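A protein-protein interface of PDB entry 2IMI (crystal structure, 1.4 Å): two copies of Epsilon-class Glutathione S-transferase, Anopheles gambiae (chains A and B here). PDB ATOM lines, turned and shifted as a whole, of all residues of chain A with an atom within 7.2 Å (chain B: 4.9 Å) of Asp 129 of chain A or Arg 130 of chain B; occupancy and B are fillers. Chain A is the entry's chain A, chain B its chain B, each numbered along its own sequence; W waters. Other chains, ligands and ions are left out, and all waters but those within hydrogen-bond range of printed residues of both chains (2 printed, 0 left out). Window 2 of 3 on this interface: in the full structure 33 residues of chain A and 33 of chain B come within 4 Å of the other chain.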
ATOM      1  N   PHE A 113       4.206 -14.264  -4.171  1.00  0.00           N
ATOM      2  CA  PHE A 113       4.713 -14.705  -5.478  1.00  0.00           C
ATOM      3  C   PHE A 113       6.149 -14.217  -5.700  1.00  0.00           C
ATOM      4  O   PHE A 113       6.875 -14.793  -6.521  1.00  0.00           O
ATOM      5  CB  PHE A 113       3.760 -14.139  -6.546  1.00  0.00           C
ATOM      6  CG  PHE A 113       3.850 -14.774  -7.913  1.00  0.00           C
ATOM      7  CD1 PHE A 113       3.871 -13.966  -9.046  1.00  0.00           C
ATOM      8  CD2 PHE A 113       3.842 -16.153  -8.080  1.00  0.00           C
ATOM      9  CE1 PHE A 113       3.922 -14.528 -10.328  1.00  0.00           C
ATOM     10  CE2 PHE A 113       3.887 -16.718  -9.365  1.00  0.00           C
ATOM     11  CZ  PHE A 113       3.925 -15.899 -10.478  1.00  0.00           C
ATOM     12  N   ILE A 114       6.554 -13.176  -4.966  1.00  0.00           N
ATOM     13  CA  ILE A 114       7.908 -12.628  -5.024  1.00  0.00           C
ATOM     14  C   ILE A 114       8.803 -13.231  -3.953  1.00  0.00           C
ATOM     15  O   ILE A 114       9.940 -13.618  -4.233  1.00  0.00           O
ATOM     16  CB  ILE A 114       7.884 -11.094  -4.862  1.00  0.00           C
ATOM     17  CG1 ILE A 114       6.957 -10.503  -5.918  1.00  0.00           C
ATOM     18  CG2 ILE A 114       9.276 -10.494  -4.996  1.00  0.00           C
ATOM     19  CD1 ILE A 114       7.425  -9.180  -6.511  1.00  0.00           C
ATOM     20  N   ILE A 126      14.364 -11.524  -8.736  1.00  0.00           N
ATOM     21  CA  ILE A 126      12.984 -11.065  -8.676  1.00  0.00           C
ATOM     22  C   ILE A 126      12.593 -10.822 -10.133  1.00  0.00           C
ATOM     23  O   ILE A 126      12.891  -9.761 -10.678  1.00  0.00           O
ATOM     24  CB  ILE A 126      12.848  -9.783  -7.832  1.00  0.00           C
ATOM     25  CG1 ILE A 126      13.347 -10.027  -6.401  1.00  0.00           C
ATOM     26  CG2 ILE A 126      11.411  -9.292  -7.830  1.00  0.00           C
ATOM     27  CD1 ILE A 126      13.545  -8.753  -5.591  1.00  0.00           C
ATOM     28  N   PRO A 127      11.972 -11.820 -10.785  1.00  0.00           N
ATOM     29  CA  PRO A 127      11.703 -11.724 -12.216  1.00  0.00           C
ATOM     30  C   PRO A 127      10.868 -10.512 -12.587  1.00  0.00           C
ATOM     31  O   PRO A 127      10.039 -10.044 -11.793  1.00  0.00           O
ATOM     32  CB  PRO A 127      10.943 -13.021 -12.521  1.00  0.00           C
ATOM     33  CG  PRO A 127      11.404 -13.974 -11.458  1.00  0.00           C
ATOM     34  CD  PRO A 127      11.505 -13.106 -10.236  1.00  0.00           C
ATOM     35  N   GLU A 128      11.098 -10.007 -13.794  1.00  0.00           N
ATOM     36  CA  GLU A 128      10.380  -8.852 -14.314  1.00  0.00           C
ATOM     37  C   GLU A 128       8.875  -8.968 -14.101  1.00  0.00           C
ATOM     38  O   GLU A 128       8.235  -7.989 -13.714  1.00  0.00           O
ATOM     39  CB  GLU A 128      10.681  -8.688 -15.808  1.00  0.00           C
ATOM     40  CG  GLU A 128      10.200  -7.382 -16.438  1.00  0.00           C
ATOM     41  CD  GLU A 128      11.252  -6.288 -16.413  1.00  0.00           C
ATOM     42  OE1 GLU A 128      11.252  -5.427 -17.322  1.00  0.00           O
ATOM     43  OE2 GLU A 128      12.096  -6.299 -15.493  1.00  0.00           O
ATOM     44  N   ASP A 129       8.309 -10.148 -14.354  1.00  0.00           N
ATOM     45  CA  ASP A 129       6.859 -10.320 -14.225  1.00  0.00           C
ATOM     46  C   ASP A 129       6.376 -10.148 -12.784  1.00  0.00           C
ATOM     47  O   ASP A 129       5.269  -9.666 -12.565  1.00  0.00           O
ATOM     48  CB  ASP A 129       6.346 -11.633 -14.870  1.00  0.00           C
ATOM     49  CG  ASP A 129       7.013 -12.898 -14.318  1.00  0.00           C
ATOM     50  OD1 ASP A 129       7.795 -12.846 -13.348  1.00  0.00           O
ATOM     51  OD2 ASP A 129       6.725 -13.993 -14.866  1.00  0.00           O
ATOM     52  N   ARG A 130       7.200 -10.542 -11.818  1.00  0.00           N
ATOM     53  CA  ARG A 130       6.911 -10.310 -10.393  1.00  0.00           C
ATOM     54  C   ARG A 130       6.902  -8.826 -10.089  1.00  0.00           C
ATOM     55  O   ARG A 130       6.006  -8.335  -9.412  1.00  0.00           O
ATOM     56  CB  ARG A 130       7.955 -10.980  -9.490  1.00  0.00           C
ATOM     57  CG  ARG A 130       7.587 -12.335  -8.946  1.00  0.00           C
ATOM     58  CD  ARG A 130       7.504 -13.317 -10.067  1.00  0.00           C
ATOM     59  NE  ARG A 130       7.385 -14.689  -9.612  1.00  0.00           N
ATOM     60  CZ  ARG A 130       7.506 -15.734 -10.418  1.00  0.00           C
ATOM     61  NH1 ARG A 130       7.387 -16.957  -9.939  1.00  0.00           N
ATOM     62  NH2 ARG A 130       7.764 -15.556 -11.703  1.00  0.00           N
ATOM     63  N   VAL A 131       7.933  -8.129 -10.555  1.00  0.00           N
ATOM     64  CA  VAL A 131       8.066  -6.693 -10.330  1.00  0.00           C
ATOM     65  C   VAL A 131       6.858  -5.966 -10.904  1.00  0.00           C
ATOM     66  O   VAL A 131       6.279  -5.113 -10.234  1.00  0.00           O
ATOM     67  CB  VAL A 131       9.370  -6.157 -10.981  1.00  0.00           C
ATOM     68  CG1 VAL A 131       9.455  -4.634 -10.879  1.00  0.00           C
ATOM     69  CG2 VAL A 131      10.592  -6.794 -10.348  1.00  0.00           C
ATOM     70  N   GLU A 132       6.473  -6.320 -12.130  1.00  0.00           N
ATOM     71  CA  GLU A 132       5.330  -5.708 -12.806  1.00  0.00           C
ATOM     72  C   GLU A 132       4.057  -5.914 -12.002  1.00  0.00           C
ATOM     73  O   GLU A 132       3.278  -4.981 -11.816  1.00  0.00           O
ATOM     74  CB  GLU A 132       5.133  -6.314 -14.202  1.00  0.00           C
ATOM     75  CG  GLU A 132       6.246  -6.034 -15.203  1.00  0.00           C
ATOM     76  CD  GLU A 132       6.200  -6.957 -16.425  1.00  0.00           C
ATOM     77  OE1 GLU A 132       5.340  -7.873 -16.495  1.00  0.00           O
ATOM     78  OE2 GLU A 132       7.045  -6.770 -17.325  1.00  0.00           O
ATOM     79  N   TYR A 133       3.844  -7.139 -11.537  1.00  0.00           N
ATOM     80  CA  TYR A 133       2.656  -7.454 -10.747  1.00  0.00           C
ATOM     81  C   TYR A 133       2.597  -6.650  -9.458  1.00  0.00           C
ATOM     82  O   TYR A 133       1.533  -6.156  -9.077  1.00  0.00           O
ATOM     83  CB  TYR A 133       2.593  -8.945 -10.408  1.00  0.00           C
ATOM     84  CG  TYR A 133       1.663  -9.741 -11.285  1.00  0.00           C
ATOM     85  CD1 TYR A 133       0.334  -9.345 -11.473  1.00  0.00           C
ATOM     86  CD2 TYR A 133       2.112 -10.891 -11.939  1.00  0.00           C
ATOM     87  CE1 TYR A 133      -0.537 -10.087 -12.276  1.00  0.00           C
ATOM     88  CE2 TYR A 133       1.255 -11.637 -12.752  1.00  0.00           C
ATOM     89  CZ  TYR A 133      -0.060 -11.227 -12.922  1.00  0.00           C
ATOM     90  OH  TYR A 133      -0.900 -11.965 -13.731  1.00  0.00           O
ATOM     91  N   VAL A 134       3.732  -6.517  -8.779  1.00  0.00           N
ATOM     92  CA  VAL A 134       3.778  -5.770  -7.529  1.00  0.00           C
ATOM     93  C   VAL A 134       3.585  -4.278  -7.789  1.00  0.00           C
ATOM     94  O   VAL A 134       2.829  -3.613  -7.078  1.00  0.00           O
ATOM     95  CB  VAL A 134       5.071  -6.048  -6.746  1.00  0.00           C
ATOM     96  CG1 VAL A 134       5.183  -5.091  -5.565  1.00  0.00           C
ATOM     97  CG2 VAL A 134       5.043  -7.469  -6.242  1.00  0.00           C
ATOM     98  N   GLN A 135       4.231  -3.735  -8.818  1.00  0.00           N
ATOM     99  CA  GLN A 135       4.017  -2.323  -9.131  1.00  0.00           C
ATOM    100  C   GLN A 135       2.554  -2.050  -9.455  1.00  0.00           C
ATOM    101  O   GLN A 135       2.005  -1.027  -9.045  1.00  0.00           O
ATOM    102  CB  GLN A 135       4.922  -1.858 -10.278  1.00  0.00           C
ATOM    103  CG  GLN A 135       6.414  -1.808  -9.938  1.00  0.00           C
ATOM    104  CD  GLN A 135       6.819  -0.733  -8.927  1.00  0.00           C
ATOM    105  OE1 GLN A 135       7.966  -0.727  -8.467  1.00  0.00           O
ATOM    106  NE2 GLN A 135       5.904   0.156  -8.571  1.00  0.00           N
ATOM    107  N   PHE B 113      -2.380 -15.795 -12.100  1.00  0.00           N
ATOM    108  CA  PHE B 113      -0.946 -15.822 -12.419  1.00  0.00           C
ATOM    109  C   PHE B 113      -0.658 -16.691 -13.642  1.00  0.00           C
ATOM    110  O   PHE B 113       0.323 -16.457 -14.340  1.00  0.00           O
ATOM    111  CB  PHE B 113      -0.100 -16.353 -11.253  1.00  0.00           C
ATOM    112  CG  PHE B 113       0.017 -15.426 -10.083  1.00  0.00           C
ATOM    113  CD1 PHE B 113       0.068 -15.956  -8.799  1.00  0.00           C
ATOM    114  CD2 PHE B 113       0.110 -14.048 -10.242  1.00  0.00           C
ATOM    115  CE1 PHE B 113       0.192 -15.126  -7.678  1.00  0.00           C
ATOM    116  CE2 PHE B 113       0.234 -13.216  -9.126  1.00  0.00           C
ATOM    117  CZ  PHE B 113       0.266 -13.766  -7.849  1.00  0.00           C
ATOM    118  N   ILE B 114      -1.492 -17.701 -13.877  1.00  0.00           N
ATOM    119  CA  ILE B 114      -1.346 -18.568 -15.036  1.00  0.00           C
ATOM    120  C   ILE B 114      -2.014 -17.991 -16.287  1.00  0.00           C
ATOM    121  O   ILE B 114      -1.438 -18.032 -17.380  1.00  0.00           O
ATOM    122  CB  ILE B 114      -1.931 -19.962 -14.743  1.00  0.00           C
ATOM    123  CG1 ILE B 114      -1.286 -20.527 -13.493  1.00  0.00           C
ATOM    124  CG2 ILE B 114      -1.709 -20.919 -15.913  1.00  0.00           C
ATOM    125  CD1 ILE B 114      -1.112 -22.040 -13.532  1.00  0.00           C
ATOM    126  N   ARG B 117      -1.281 -13.687 -18.300  1.00  0.00           N
ATOM    127  CA  ARG B 117      -0.184 -13.477 -19.240  1.00  0.00           C
ATOM    128  C   ARG B 117      -0.514 -14.056 -20.615  1.00  0.00           C
ATOM    129  O   ARG B 117      -0.069 -13.526 -21.636  1.00  0.00           O
ATOM    130  CB  ARG B 117       1.133 -14.027 -18.695  1.00  0.00           C
ATOM    131  CG  ARG B 117       1.107 -15.503 -18.326  1.00  0.00           C
ATOM    132  CD  ARG B 117       2.289 -15.893 -17.433  1.00  0.00           C
ATOM    133  NE  ARG B 117       3.580 -15.703 -18.103  1.00  0.00           N
ATOM    134  CZ  ARG B 117       4.058 -16.506 -19.052  1.00  0.00           C
ATOM    135  NH1 ARG B 117       3.353 -17.555 -19.465  1.00  0.00           N
ATOM    136  NH2 ARG B 117       5.239 -16.259 -19.601  1.00  0.00           N
ATOM    137  N   ILE B 126       3.116 -22.096 -20.411  1.00  0.00           N
ATOM    138  CA  ILE B 126       2.742 -22.168 -19.008  1.00  0.00           C
ATOM    139  C   ILE B 126       3.997 -22.600 -18.256  1.00  0.00           C
ATOM    140  O   ILE B 126       4.346 -23.781 -18.270  1.00  0.00           O
ATOM    141  CB  ILE B 126       1.597 -23.178 -18.746  1.00  0.00           C
ATOM    142  CG1 ILE B 126       0.420 -22.958 -19.705  1.00  0.00           C
ATOM    143  CG2 ILE B 126       1.129 -23.080 -17.289  1.00  0.00           C
ATOM    144  CD1 ILE B 126      -0.506 -24.173 -19.856  1.00  0.00           C
ATOM    145  N   PRO B 127       4.709 -21.641 -17.635  1.00  0.00           N
ATOM    146  CA  PRO B 127       5.939 -21.994 -16.928  1.00  0.00           C
ATOM    147  C   PRO B 127       5.724 -23.039 -15.843  1.00  0.00           C
ATOM    148  O   PRO B 127       4.660 -23.094 -15.216  1.00  0.00           O
ATOM    149  CB  PRO B 127       6.385 -20.667 -16.317  1.00  0.00           C
ATOM    150  CG  PRO B 127       5.812 -19.639 -17.236  1.00  0.00           C
ATOM    151  CD  PRO B 127       4.461 -20.190 -17.583  1.00  0.00           C
ATOM    152  N   GLU B 128       6.743 -23.858 -15.628  1.00  0.00           N
ATOM    153  CA  GLU B 128       6.663 -24.972 -14.698  1.00  0.00           C
ATOM    154  C   GLU B 128       6.293 -24.511 -13.293  1.00  0.00           C
ATOM    155  O   GLU B 128       5.532 -25.182 -12.598  1.00  0.00           O
ATOM    156  CB  GLU B 128       7.989 -25.737 -14.687  1.00  0.00           C
ATOM    157  CG  GLU B 128       8.332 -26.441 -16.017  1.00  0.00           C
ATOM    158  CD  GLU B 128       8.753 -25.495 -17.159  1.00  0.00           C
ATOM    159  OE1 GLU B 128       8.720 -25.944 -18.330  1.00  0.00           O
ATOM    160  OE2 GLU B 128       9.121 -24.320 -16.906  1.00  0.00           O
ATOM    161  N   ASP B 129       6.806 -23.356 -12.878  1.00  0.00           N
ATOM    162  CA  ASP B 129       6.510 -22.850 -11.535  1.00  0.00           C
ATOM    163  C   ASP B 129       5.024 -22.499 -11.347  1.00  0.00           C
ATOM    164  O   ASP B 129       4.490 -22.625 -10.238  1.00  0.00           O
ATOM    165  CB  ASP B 129       7.466 -21.710 -11.116  1.00  0.00           C
ATOM    166  CG  ASP B 129       7.309 -20.442 -11.944  1.00  0.00           C
ATOM    167  OD1 ASP B 129       8.010 -19.456 -11.621  1.00  0.00           O
ATOM    168  OD2 ASP B 129       6.497 -20.391 -12.896  1.00  0.00           O
ATOM    169  N   ARG B 130       4.361 -22.098 -12.435  1.00  0.00           N
ATOM    170  CA  ARG B 130       2.929 -21.791 -12.407  1.00  0.00           C
ATOM    171  C   ARG B 130       2.123 -23.073 -12.219  1.00  0.00           C
ATOM    172  O   ARG B 130       1.194 -23.108 -11.414  1.00  0.00           O
ATOM    173  CB  ARG B 130       2.481 -21.092 -13.701  1.00  0.00           C
ATOM    174  CG  ARG B 130       3.218 -19.820 -14.082  1.00  0.00           C
ATOM    175  CD  ARG B 130       3.036 -18.715 -13.064  1.00  0.00           C
ATOM    176  NE  ARG B 130       3.255 -17.383 -13.633  1.00  0.00           N
ATOM    177  CZ  ARG B 130       4.445 -16.863 -13.923  1.00  0.00           C
ATOM    178  NH1 ARG B 130       5.555 -17.558 -13.720  1.00  0.00           N
ATOM    179  NH2 ARG B 130       4.525 -15.642 -14.425  1.00  0.00           N
ATOM    180  N   VAL B 131       2.493 -24.115 -12.962  1.00  0.00           N
ATOM    181  CA  VAL B 131       1.857 -25.431 -12.860  1.00  0.00           C
ATOM    182  C   VAL B 131       1.973 -25.945 -11.430  1.00  0.00           C
ATOM    183  O   VAL B 131       0.987 -26.368 -10.828  1.00  0.00           O
ATOM    184  CB  VAL B 131       2.466 -26.455 -13.867  1.00  0.00           C
ATOM    185  CG1 VAL B 131       1.909 -27.853 -13.624  1.00  0.00           C
ATOM    186  CG2 VAL B 131       2.193 -26.019 -15.300  1.00  0.00           C
ATOM    187  N   GLU B 132       3.173 -25.862 -10.870  1.00  0.00           N
ATOM    188  CA  GLU B 132       3.413 -26.358  -9.521  1.00  0.00           C
ATOM    189  C   GLU B 132       2.606 -25.576  -8.493  1.00  0.00           C
ATOM    190  O   GLU B 132       2.038 -26.164  -7.574  1.00  0.00           O
ATOM    191  CB  GLU B 132       4.904 -26.304  -9.193  1.00  0.00           C
ATOM    192  CG  GLU B 132       5.719 -27.363  -9.927  1.00  0.00           C
ATOM    193  CD  GLU B 132       7.205 -27.285  -9.622  1.00  0.00           C
ATOM    194  OE1 GLU B 132       7.773 -26.172  -9.668  1.00  0.00           O
ATOM    195  OE2 GLU B 132       7.810 -28.347  -9.352  1.00  0.00           O
ATOM    196  N   TYR B 133       2.539 -24.260  -8.665  1.00  0.00           N
ATOM    197  CA  TYR B 133       1.793 -23.406  -7.753  1.00  0.00           C
ATOM    198  C   TYR B 133       0.311 -23.782  -7.766  1.00  0.00           C
ATOM    199  O   TYR B 133      -0.335 -23.850  -6.718  1.00  0.00           O
ATOM    200  CB  TYR B 133       1.981 -21.939  -8.165  1.00  0.00           C
ATOM    201  CG  TYR B 133       2.275 -20.962  -7.049  1.00  0.00           C
ATOM    202  CD1 TYR B 133       2.037 -19.605  -7.230  1.00  0.00           C
ATOM    203  CD2 TYR B 133       2.769 -21.387  -5.818  1.00  0.00           C
ATOM    204  CE1 TYR B 133       2.299 -18.690  -6.223  1.00  0.00           C
ATOM    205  CE2 TYR B 133       3.037 -20.476  -4.798  1.00  0.00           C
ATOM    206  CZ  TYR B 133       2.800 -19.138  -5.012  1.00  0.00           C
ATOM    207  OH  TYR B 133       3.068 -18.239  -4.001  1.00  0.00           O
ATOM    208  N   VAL B 134      -0.220 -24.026  -8.960  1.00  0.00           N
ATOM    209  CA  VAL B 134      -1.628 -24.404  -9.109  1.00  0.00           C
ATOM    210  C   VAL B 134      -1.897 -25.805  -8.545  1.00  0.00           C
ATOM    211  O   VAL B 134      -2.879 -26.018  -7.826  1.00  0.00           O
ATOM    212  CB  VAL B 134      -2.088 -24.254 -10.565  1.00  0.00           C
ATOM    213  CG1 VAL B 134      -3.441 -24.908 -10.770  1.00  0.00           C
ATOM    214  CG2 VAL B 134      -2.158 -22.773 -10.920  1.00  0.00           C
HETATM  215  O   HOH W   1      -0.202 -13.999 -15.600  1.00  0.00           O
HETATM  216  O   HOH W   2       5.870 -13.921 -17.522  1.00  0.00           O
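The guanidinium group (NH2) of Arg 130 of chain B lies within salt-bridge range of the side-chain carboxylate (OD2) of Asp 129 of chain A (2.8 Å).
NH1 of Arg 130 of chain A lies within salt-bridge range of OD1 of Asp 129 of chain B (3.1 Å).
NE of Arg 130 of chain A lies within hydrogen-bond range of O of Phe 113 of chain A (3.1 Å).
The guanidinium group (NH2) of Arg 130 of chain A lies within salt-bridge range of the side-chain carboxylate (OD1) of Asp 129 of chain A, 3.2 Å away.
The backbone carbonyl oxygen of Phe 113 of chain B is in hydrogen-bond range of the guanidinium group of Arg 130 of chain B, at 3.2 Å.
OD2 of Asp 129 of chain B lies within salt-bridge range of NH1 of Arg 130 of chain B (3.1 Å).
CG of Phe 113 of chain A touches CE1 of Phe 113 of chain B (3.7 Å).
CZ of Phe 113 of chain A touches NE of Arg 130 of chain B, 3.6 Å away.
CD2 of Phe 113 of chain A touches CE1 of Tyr 133 of chain B, at 3.5 Å.
NH2 of Arg 130 of chain A touches NH1 of Arg 130 of chain B (3.6 Å).
Tyr 133 of chain A touches Phe 113 of chain B (CE2 to CD2, 3.7 Å).
Of the printed residues of chain B, Phe 113 of chain A touches Phe 113 (3.7 Å), Arg 130 (3.6 Å) and Tyr 133 (3.5 Å).
Ile 114 of chain A touches none of the printed residues of chain B.
Asp 129 of chain A touches one residue of chain B.
Printed residues of chain B within 4 Å of Arg 130 of chain A: Asp 129 and Arg 130.
Glu 132 of chain A touches none of the printed residues of chain B.
Printed residues of chain B within 4 Å of Tyr 133 of chain A: Phe 113 (3.7 Å).
Printed residues of chain A within 4 Å of Phe 113 of chain B: Phe 113 and Tyr 133.
Printed residues of chain A within 4 Å of Asp 129 of chain B: Arg 130.
Arg 130 of chain B touches just these residues of chain A: Phe 113 (3.6 Å), Asp 129 (2.8 Å) and Arg 130 (3.6 Å).
The nearest residue of chain A that does not touch Arg 130 of chain B is Tyr 133 of chain A (5.4 Å).
The nearest printed residue of chain B that does not touch Tyr 133 of chain A is Arg 117 of chain B (4.9 Å).
Of the 12 printed residues of chain A, 4 touch a printed residue of chain B.
Of the 12 printed residues of chain B, 4 touch a printed residue of chain A.
Hydrophobic or aromatic side chains of chain B that line the printed part of chain A: Phe 113 and Tyr 133.
Among the printed residues, 7 pairs touch across the chains.
Phe 113 of chain A touches Arg 130 of chain B, but with the chains exchanged Arg 130 of chain A does not touch Phe 113 of chain B (7.3 Å).
Phe 113 of chain A touches Tyr 133 of chain B, and with the chains exchanged Tyr 133 of chain A touches Phe 113 of chain B.
Asp 129 of chain A touches Arg 130 of chain B, and with the chains exchanged Arg 130 of chain A touches Asp 129 of chain B.
Arg 130 of chain A touches its own counterpart, Arg 130 of chain B.
Positions printed for both chains: 113, 114, 126, 127, 128, 129, 130, 131, 132, 133 and 134.
Of the 7 pairs that touch across the chains among the printed residues, 6 have their exchanged pair printed and touching as well.
Water W2 lies within hydrogen-bond range of OD2 of Asp 129 of chain A (2.8 Å) and NE of Arg 117 of chain B (3.0 Å).
Water W1 lies within hydrogen-bond range of the backbone carbonyl oxygen of Phe 113 of chain B (2.8 Å), the side-chain hydroxyl of Tyr 133 of chain A (2.8 Å) and the backbone NH of Arg 117 of chain B (2.9 Å).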
